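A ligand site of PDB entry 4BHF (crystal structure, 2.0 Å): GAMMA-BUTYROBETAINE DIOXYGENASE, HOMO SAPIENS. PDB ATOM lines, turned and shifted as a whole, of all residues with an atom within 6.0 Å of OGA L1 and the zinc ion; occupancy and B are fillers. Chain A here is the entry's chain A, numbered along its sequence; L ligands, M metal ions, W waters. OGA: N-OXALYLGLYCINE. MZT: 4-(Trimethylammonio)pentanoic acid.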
ATOM      1  N   TRP A 181      26.853  18.570  36.668  1.00  0.00           N
ATOM      2  CA  TRP A 181      26.669  17.984  35.336  1.00  0.00           C
ATOM      3  C   TRP A 181      27.843  18.275  34.437  1.00  0.00           C
ATOM      4  O   TRP A 181      28.561  19.246  34.665  1.00  0.00           O
ATOM      5  CB  TRP A 181      25.375  18.478  34.668  1.00  0.00           C
ATOM      6  CG  TRP A 181      24.862  19.783  35.137  1.00  0.00           C
ATOM      7  CD1 TRP A 181      23.948  20.010  36.128  1.00  0.00           C
ATOM      8  CD2 TRP A 181      25.207  21.079  34.614  1.00  0.00           C
ATOM      9  NE1 TRP A 181      23.735  21.342  36.272  1.00  0.00           N
ATOM     10  CE2 TRP A 181      24.504  22.029  35.365  1.00  0.00           C
ATOM     11  CE3 TRP A 181      26.032  21.522  33.573  1.00  0.00           C
ATOM     12  CZ2 TRP A 181      24.598  23.386  35.113  1.00  0.00           C
ATOM     13  CZ3 TRP A 181      26.125  22.865  33.331  1.00  0.00           C
ATOM     14  CH2 TRP A 181      25.414  23.791  34.099  1.00  0.00           C
ATOM     15  N   VAL A 183      29.411  19.214  30.833  1.00  0.00           N
ATOM     16  CA  VAL A 183      29.232  19.793  29.509  1.00  0.00           C
ATOM     17  C   VAL A 183      30.362  19.251  28.635  1.00  0.00           C
ATOM     18  O   VAL A 183      31.517  19.671  28.754  1.00  0.00           O
ATOM     19  CB  VAL A 183      29.279  21.321  29.525  1.00  0.00           C
ATOM     20  CG1 VAL A 183      28.966  21.873  28.153  1.00  0.00           C
ATOM     21  CG2 VAL A 183      28.323  21.876  30.571  1.00  0.00           C
ATOM     22  N   ASN A 191      20.515  17.159  25.130  1.00  0.00           N
ATOM     23  CA  ASN A 191      20.522  18.608  25.231  1.00  0.00           C
ATOM     24  C   ASN A 191      21.564  19.192  24.285  1.00  0.00           C
ATOM     25  O   ASN A 191      22.681  18.679  24.214  1.00  0.00           O
ATOM     26  CB  ASN A 191      20.891  19.010  26.661  1.00  0.00           C
ATOM     27  CG  ASN A 191      20.481  20.435  26.995  1.00  0.00           C
ATOM     28  OD1 ASN A 191      21.142  21.403  26.583  1.00  0.00           O
ATOM     29  ND2 ASN A 191      19.390  20.564  27.741  1.00  0.00           N
ATOM     30  N   ALA A 193      23.414  21.591  24.652  1.00  0.00           N
ATOM     31  CA  ALA A 193      24.626  21.906  25.412  1.00  0.00           C
ATOM     32  C   ALA A 193      25.653  20.772  25.309  1.00  0.00           C
ATOM     33  O   ALA A 193      26.841  21.012  25.272  1.00  0.00           O
ATOM     34  CB  ALA A 193      24.274  22.178  26.862  1.00  0.00           C
ATOM     35  N   TYR A 194      25.166  19.541  25.214  1.00  0.00           N
ATOM     36  CA  TYR A 194      26.046  18.357  25.223  1.00  0.00           C
ATOM     37  C   TYR A 194      26.449  17.907  23.788  1.00  0.00           C
ATOM     38  O   TYR A 194      26.480  16.729  23.461  1.00  0.00           O
ATOM     39  CB  TYR A 194      25.349  17.240  25.998  1.00  0.00           C
ATOM     40  CG  TYR A 194      25.027  17.578  27.488  1.00  0.00           C
ATOM     41  CD1 TYR A 194      25.766  18.524  28.231  1.00  0.00           C
ATOM     42  CD2 TYR A 194      24.010  16.888  28.146  1.00  0.00           C
ATOM     43  CE1 TYR A 194      25.460  18.785  29.565  1.00  0.00           C
ATOM     44  CE2 TYR A 194      23.704  17.132  29.467  1.00  0.00           C
ATOM     45  CZ  TYR A 194      24.422  18.084  30.171  1.00  0.00           C
ATOM     46  OH  TYR A 194      24.091  18.283  31.481  1.00  0.00           O
ATOM     47  N   LEU A 199      26.368  27.716  20.943  1.00  0.00           N
ATOM     48  CA  LEU A 199      25.199  28.123  21.726  1.00  0.00           C
ATOM     49  C   LEU A 199      25.104  29.624  21.627  1.00  0.00           C
ATOM     50  O   LEU A 199      26.017  30.349  22.014  1.00  0.00           O
ATOM     51  CB  LEU A 199      25.342  27.681  23.199  1.00  0.00           C
ATOM     52  CG  LEU A 199      25.511  26.176  23.435  1.00  0.00           C
ATOM     53  CD1 LEU A 199      25.760  25.839  24.896  1.00  0.00           C
ATOM     54  CD2 LEU A 199      24.305  25.429  22.938  1.00  0.00           C
ATOM     55  N   HIS A 202      21.664  32.710  25.696  1.00  0.00           N
ATOM     56  CA  HIS A 202      20.555  32.105  26.398  1.00  0.00           C
ATOM     57  C   HIS A 202      20.759  32.236  27.915  1.00  0.00           C
ATOM     58  O   HIS A 202      21.888  32.467  28.375  1.00  0.00           O
ATOM     59  CB  HIS A 202      20.439  30.622  26.032  1.00  0.00           C
ATOM     60  CG  HIS A 202      21.585  29.768  26.483  1.00  0.00           C
ATOM     61  ND1 HIS A 202      22.795  29.762  25.835  1.00  0.00           N
ATOM     62  CD2 HIS A 202      21.697  28.885  27.507  1.00  0.00           C
ATOM     63  CE1 HIS A 202      23.614  28.905  26.436  1.00  0.00           C
ATOM     64  NE2 HIS A 202      22.966  28.352  27.443  1.00  0.00           N
ATOM     65  N   THR A 203      19.655  32.129  28.638  1.00  0.00           N
ATOM     66  CA  THR A 203      19.662  31.768  30.062  1.00  0.00           C
ATOM     67  C   THR A 203      19.404  30.260  30.170  1.00  0.00           C
ATOM     68  O   THR A 203      18.774  29.701  29.288  1.00  0.00           O
ATOM     69  CB  THR A 203      18.591  32.523  30.853  1.00  0.00           C
ATOM     70  OG1 THR A 203      17.277  32.299  30.313  1.00  0.00           O
ATOM     71  CG2 THR A 203      18.850  34.035  30.807  1.00  0.00           C
ATOM     72  N   ASP A 204      19.914  29.639  31.231  1.00  0.00           N
ATOM     73  CA  ASP A 204      19.663  28.242  31.540  1.00  0.00           C
ATOM     74  C   ASP A 204      18.338  28.014  32.206  1.00  0.00           C
ATOM     75  O   ASP A 204      17.868  28.774  33.075  1.00  0.00           O
ATOM     76  CB  ASP A 204      20.787  27.672  32.436  1.00  0.00           C
ATOM     77  CG  ASP A 204      21.946  27.110  31.642  1.00  0.00           C
ATOM     78  OD1 ASP A 204      22.224  27.672  30.562  1.00  0.00           O
ATOM     79  OD2 ASP A 204      22.564  26.110  32.100  1.00  0.00           O
ATOM     80  N   GLN A 215      24.610  30.340  38.308  1.00  0.00           N
ATOM     81  CA  GLN A 215      25.195  29.242  37.617  1.00  0.00           C
ATOM     82  C   GLN A 215      26.705  29.225  37.851  1.00  0.00           C
ATOM     83  O   GLN A 215      27.332  30.254  37.924  1.00  0.00           O
ATOM     84  CB  GLN A 215      24.903  29.352  36.126  1.00  0.00           C
ATOM     85  CG  GLN A 215      25.572  28.285  35.289  1.00  0.00           C
ATOM     86  CD  GLN A 215      25.021  28.164  33.861  1.00  0.00           C
ATOM     87  OE1 GLN A 215      25.673  27.570  33.002  1.00  0.00           O
ATOM     88  NE2 GLN A 215      23.841  28.723  33.610  1.00  0.00           N
ATOM     89  N   LEU A 217      30.274  27.352  36.370  1.00  0.00           N
ATOM     90  CA  LEU A 217      30.856  26.580  35.260  1.00  0.00           C
ATOM     91  C   LEU A 217      32.377  26.534  35.437  1.00  0.00           C
ATOM     92  O   LEU A 217      33.053  27.566  35.496  1.00  0.00           O
ATOM     93  CB  LEU A 217      30.527  27.202  33.884  1.00  0.00           C
ATOM     94  CG  LEU A 217      29.218  26.982  33.103  1.00  0.00           C
ATOM     95  CD1 LEU A 217      29.288  27.727  31.763  1.00  0.00           C
ATOM     96  CD2 LEU A 217      29.016  25.527  32.827  1.00  0.00           C
ATOM     97  N   GLY A 227      35.095  27.129  21.068  1.00  0.00           N
ATOM     98  CA  GLY A 227      34.584  27.000  22.449  1.00  0.00           C
ATOM     99  C   GLY A 227      34.855  28.190  23.357  1.00  0.00           C
ATOM    100  O   GLY A 227      34.745  28.083  24.567  1.00  0.00           O
ATOM    101  N   ASP A 228      35.173  29.339  22.774  1.00  0.00           N
ATOM    102  CA  ASP A 228      35.186  30.613  23.510  1.00  0.00           C
ATOM    103  C   ASP A 228      33.838  30.871  24.151  1.00  0.00           C
ATOM    104  O   ASP A 228      32.807  30.465  23.618  1.00  0.00           O
ATOM    105  CB  ASP A 228      35.490  31.791  22.577  1.00  0.00           C
ATOM    106  CG  ASP A 228      36.795  31.584  21.801  1.00  0.00           C
ATOM    107  OD1 ASP A 228      36.793  30.779  20.842  1.00  0.00           O
ATOM    108  OD2 ASP A 228      37.808  32.174  22.195  1.00  0.00           O
ATOM    109  N   SER A 229      33.852  31.581  25.280  1.00  0.00           N
ATOM    110  CA  SER A 229      32.648  31.993  25.965  1.00  0.00           C
ATOM    111  C   SER A 229      32.219  33.393  25.585  1.00  0.00           C
ATOM    112  O   SER A 229      33.053  34.239  25.256  1.00  0.00           O
ATOM    113  CB  SER A 229      32.893  31.935  27.466  1.00  0.00           C
ATOM    114  OG  SER A 229      33.310  30.648  27.801  1.00  0.00           O
ATOM    115  N   ASN A 292      15.920  30.624  26.301  1.00  0.00           N
ATOM    116  CA  ASN A 292      16.803  29.684  25.651  1.00  0.00           C
ATOM    117  C   ASN A 292      16.111  29.249  24.323  1.00  0.00           C
ATOM    118  O   ASN A 292      14.984  28.755  24.326  1.00  0.00           O
ATOM    119  CB  ASN A 292      17.092  28.524  26.585  1.00  0.00           C
ATOM    120  CG  ASN A 292      18.083  27.540  25.994  1.00  0.00           C
ATOM    121  OD1 ASN A 292      18.326  27.553  24.769  1.00  0.00           O
ATOM    122  ND2 ASN A 292      18.645  26.708  26.812  1.00  0.00           N
ATOM    123  N   MET A 332      37.750  30.275  28.515  1.00  0.00           N
ATOM    124  CA  MET A 332      38.056  29.628  29.774  1.00  0.00           C
ATOM    125  C   MET A 332      39.254  28.676  29.590  1.00  0.00           C
ATOM    126  O   MET A 332      39.360  28.031  28.576  1.00  0.00           O
ATOM    127  CB  MET A 332      36.853  28.833  30.255  1.00  0.00           C
ATOM    128  CG  MET A 332      35.595  29.677  30.495  1.00  0.00           C
ATOM    129  SD  MET A 332      34.359  28.808  31.484  1.00  0.00           S
ATOM    130  CE  MET A 332      35.181  28.919  33.076  1.00  0.00           C
ATOM    131  N   HIS A 347      24.432  33.961  28.211  1.00  0.00           N
ATOM    132  CA  HIS A 347      25.722  33.457  27.919  1.00  0.00           C
ATOM    133  C   HIS A 347      25.626  32.506  26.731  1.00  0.00           C
ATOM    134  O   HIS A 347      24.530  32.053  26.343  1.00  0.00           O
ATOM    135  CB  HIS A 347      26.287  32.742  29.144  1.00  0.00           C
ATOM    136  CG  HIS A 347      25.518  31.525  29.550  1.00  0.00           C
ATOM    137  ND1 HIS A 347      24.331  31.596  30.247  1.00  0.00           N
ATOM    138  CD2 HIS A 347      25.785  30.210  29.374  1.00  0.00           C
ATOM    139  CE1 HIS A 347      23.881  30.371  30.472  1.00  0.00           C
ATOM    140  NE2 HIS A 347      24.750  29.513  29.958  1.00  0.00           N
ATOM    141  N   GLY A 348      26.780  32.248  26.150  1.00  0.00           N
ATOM    142  CA  GLY A 348      26.863  31.353  25.020  1.00  0.00           C
ATOM    143  C   GLY A 348      28.255  30.816  24.784  1.00  0.00           C
ATOM    144  O   GLY A 348      29.183  31.093  25.524  1.00  0.00           O
ATOM    145  N   ARG A 349      28.394  30.045  23.730  1.00  0.00           N
ATOM    146  CA  ARG A 349      29.691  29.565  23.385  1.00  0.00           C
ATOM    147  C   ARG A 349      29.791  29.322  21.872  1.00  0.00           C
ATOM    148  O   ARG A 349      28.795  29.050  21.182  1.00  0.00           O
ATOM    149  CB  ARG A 349      30.052  28.300  24.137  1.00  0.00           C
ATOM    150  CG  ARG A 349      29.268  27.087  23.688  1.00  0.00           C
ATOM    151  CD  ARG A 349      30.047  25.776  23.747  1.00  0.00           C
ATOM    152  NE  ARG A 349      29.194  24.805  23.081  1.00  0.00           N
ATOM    153  CZ  ARG A 349      28.495  23.816  23.635  1.00  0.00           C
ATOM    154  NH1 ARG A 349      28.536  23.517  24.931  1.00  0.00           N
ATOM    155  NH2 ARG A 349      27.741  23.078  22.819  1.00  0.00           N
ATOM    156  N   ARG A 360      36.935  18.719  25.261  1.00  0.00           N
ATOM    157  CA  ARG A 360      36.405  19.837  26.017  1.00  0.00           C
ATOM    158  C   ARG A 360      35.453  19.327  27.072  1.00  0.00           C
ATOM    159  O   ARG A 360      34.594  18.508  26.774  1.00  0.00           O
ATOM    160  CB  ARG A 360      35.724  20.825  25.060  1.00  0.00           C
ATOM    161  CG  ARG A 360      35.373  22.155  25.707  1.00  0.00           C
ATOM    162  CD  ARG A 360      34.633  23.027  24.721  1.00  0.00           C
ATOM    163  NE  ARG A 360      34.383  24.377  25.208  1.00  0.00           N
ATOM    164  CZ  ARG A 360      33.312  24.767  25.886  1.00  0.00           C
ATOM    165  NH1 ARG A 360      32.372  23.910  26.274  1.00  0.00           N
ATOM    166  NH2 ARG A 360      33.199  26.052  26.216  1.00  0.00           N
ATOM    167  N   LEU A 362      33.474  20.913  30.726  1.00  0.00           N
ATOM    168  CA  LEU A 362      33.212  21.774  31.874  1.00  0.00           C
ATOM    169  C   LEU A 362      32.308  21.009  32.837  1.00  0.00           C
ATOM    170  O   LEU A 362      31.480  20.201  32.401  1.00  0.00           O
ATOM    171  CB  LEU A 362      32.548  23.092  31.467  1.00  0.00           C
ATOM    172  CG  LEU A 362      32.912  23.750  30.127  1.00  0.00           C
ATOM    173  CD1 LEU A 362      31.871  24.807  29.808  1.00  0.00           C
ATOM    174  CD2 LEU A 362      34.302  24.362  30.113  1.00  0.00           C
ATOM    175  N   TYR A 366      24.116  24.651  39.731  1.00  0.00           N
ATOM    176  CA  TYR A 366      23.274  25.787  39.964  1.00  0.00           C
ATOM    177  C   TYR A 366      23.123  26.045  41.467  1.00  0.00           C
ATOM    178  O   TYR A 366      23.325  25.146  42.282  1.00  0.00           O
ATOM    179  CB  TYR A 366      21.884  25.531  39.379  1.00  0.00           C
ATOM    180  CG  TYR A 366      21.828  25.316  37.871  1.00  0.00           C
ATOM    181  CD1 TYR A 366      22.279  26.284  36.981  1.00  0.00           C
ATOM    182  CD2 TYR A 366      21.280  24.151  37.348  1.00  0.00           C
ATOM    183  CE1 TYR A 366      22.206  26.088  35.609  1.00  0.00           C
ATOM    184  CE2 TYR A 366      21.185  23.947  35.985  1.00  0.00           C
ATOM    185  CZ  TYR A 366      21.646  24.907  35.113  1.00  0.00           C
ATOM    186  OH  TYR A 366      21.552  24.686  33.736  1.00  0.00           O
HETATM  187  C1  OGA L   1      25.356  25.236  28.898  1.00  0.00           C
HETATM  188  C2  OGA L   1      26.304  26.283  28.511  1.00  0.00           C
HETATM  189  C4  OGA L   1      28.565  26.899  28.004  1.00  0.00           C
HETATM  190  C5  OGA L   1      29.746  26.262  27.339  1.00  0.00           C
HETATM  191  O1  OGA L   1      24.179  25.572  29.115  1.00  0.00           O
HETATM  192  O2  OGA L   1      25.773  24.059  29.036  1.00  0.00           O
HETATM  193  O2' OGA L   1      25.917  27.433  28.366  1.00  0.00           O
HETATM  194  O3  OGA L   1      30.700  27.023  27.196  1.00  0.00           O
HETATM  195  N1  OGA L   1      27.575  25.905  28.355  1.00  0.00           N
HETATM  196  O4  OGA L   1      29.728  25.077  26.928  1.00  0.00           O
HETATM  197  N1  MZT L   2      22.254  22.055  30.975  1.00  0.00           N
HETATM  198  C8  MZT L   2      22.311  21.620  32.389  1.00  0.00           C
HETATM  199  O4  MZT L   2      18.350  23.498  28.608  1.00  0.00           O
HETATM  200  C5  MZT L   2      18.765  24.574  29.077  1.00  0.00           C
HETATM  201  O7  MZT L   2      17.955  25.457  29.342  1.00  0.00           O
HETATM  202  C6  MZT L   2      20.231  24.917  29.332  1.00  0.00           C
HETATM  203  C2  MZT L   2      21.281  23.200  30.847  1.00  0.00           C
HETATM  204  C9  MZT L   2      23.609  22.494  30.623  1.00  0.00           C
HETATM  205  C10 MZT L   2      21.935  20.893  30.122  1.00  0.00           C
HETATM  206  C3  MZT L   2      21.159  23.712  29.409  1.00  0.00           C
HETATM  207  C21 MZT L   2      19.887  22.907  31.359  1.00  0.00           C
HETATM  208 ZN    ZN M   1      23.898  27.572  29.235  1.00  0.00          ZN
HETATM  209  O   HOH W   1      30.729  29.689  27.667  1.00  0.00           O
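The guanidinium group of Arg 349 lies within salt-bridge range of an oxygen (O4) of OGA L1, at 2.8 Å. O4 of MZT L2 lies within hydrogen-bond range of ND2 of Asn 191, at 3.2 Å. The side-chain amide nitrogen (ND2) of Asn 292 sits at hydrogen-bond distance from an oxygen (O7) of MZT L2 (2.9 Å). NH2 of Arg 360 is in salt-bridge range of O3 of OGA L1 (2.9 Å).
The backbone carbonyl oxygen (O) of Arg 349 is in hydrogen-bond range of the backbone NH (N) of Leu 199 (2.8 Å). The guanidinium group (NH1) of Arg 349 is in hydrogen-bond range of the backbone carbonyl oxygen (O) of Ala 193, at 3.0 Å. The backbone NH (N) of Ala 193 lies within hydrogen-bond range of the side-chain amide oxygen (OD1) of Asn 191 (3.0 Å). The backbone NH of Val 183 sits at hydrogen-bond distance from the backbone carbonyl oxygen of Leu 362 (2.8 Å). The side-chain carboxylate of Asp 204 lies close to the side-chain amide nitrogen of Gln 215 (3.3 Å). The guanidinium group of Arg 360 sits at hydrogen-bond distance from the backbone carbonyl oxygen of Gly 227, at 3.0 Å.
Val 183 touches OGA L1 (CG1 to O4, 3.5 Å). CB of Ala 193 touches O2 of OGA L1, 3.2 Å away. Leu 199 touches OGA L1 (CD1 to C2, 3.7 Å). Leu 217 touches OGA L1 (CD1 to C4, 3.9 Å). Leu 362 touches OGA L1. Hydrophobic or aromatic side chains that line OGA L1: Val 183, Ala 193, Leu 199, His 202, Leu 217, His 347 and Leu 362. Along chain A the residues within 4 Å of OGA L1 span positions 183 to 362. The nearest printed residue that does not touch OGA L1 is Trp 181 (4.5 Å).
Of the 22 residues printed, 3 come within 4 Å of the zinc ion.
The zinc ion is bound by O1 of OGA L1, at 2.0 Å. The zinc ion is bound by the side-chain carboxylate (OD1) of Asp 204. The zinc ion is bound by a ring nitrogen (NE2) of His 202, 2.2 Å away. The zinc ion is bound by an oxygen (O2') of OGA L1. NE2 of His 347 is bound to the zinc ion (2.2 Å). The zinc ion has five donor atoms within binding distance.
Water W1 lies within hydrogen-bond range of O3 of OGA L1 (2.7 Å), OG of Ser 229 (2.8 Å) and O of Gly 348 (3.0 Å).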
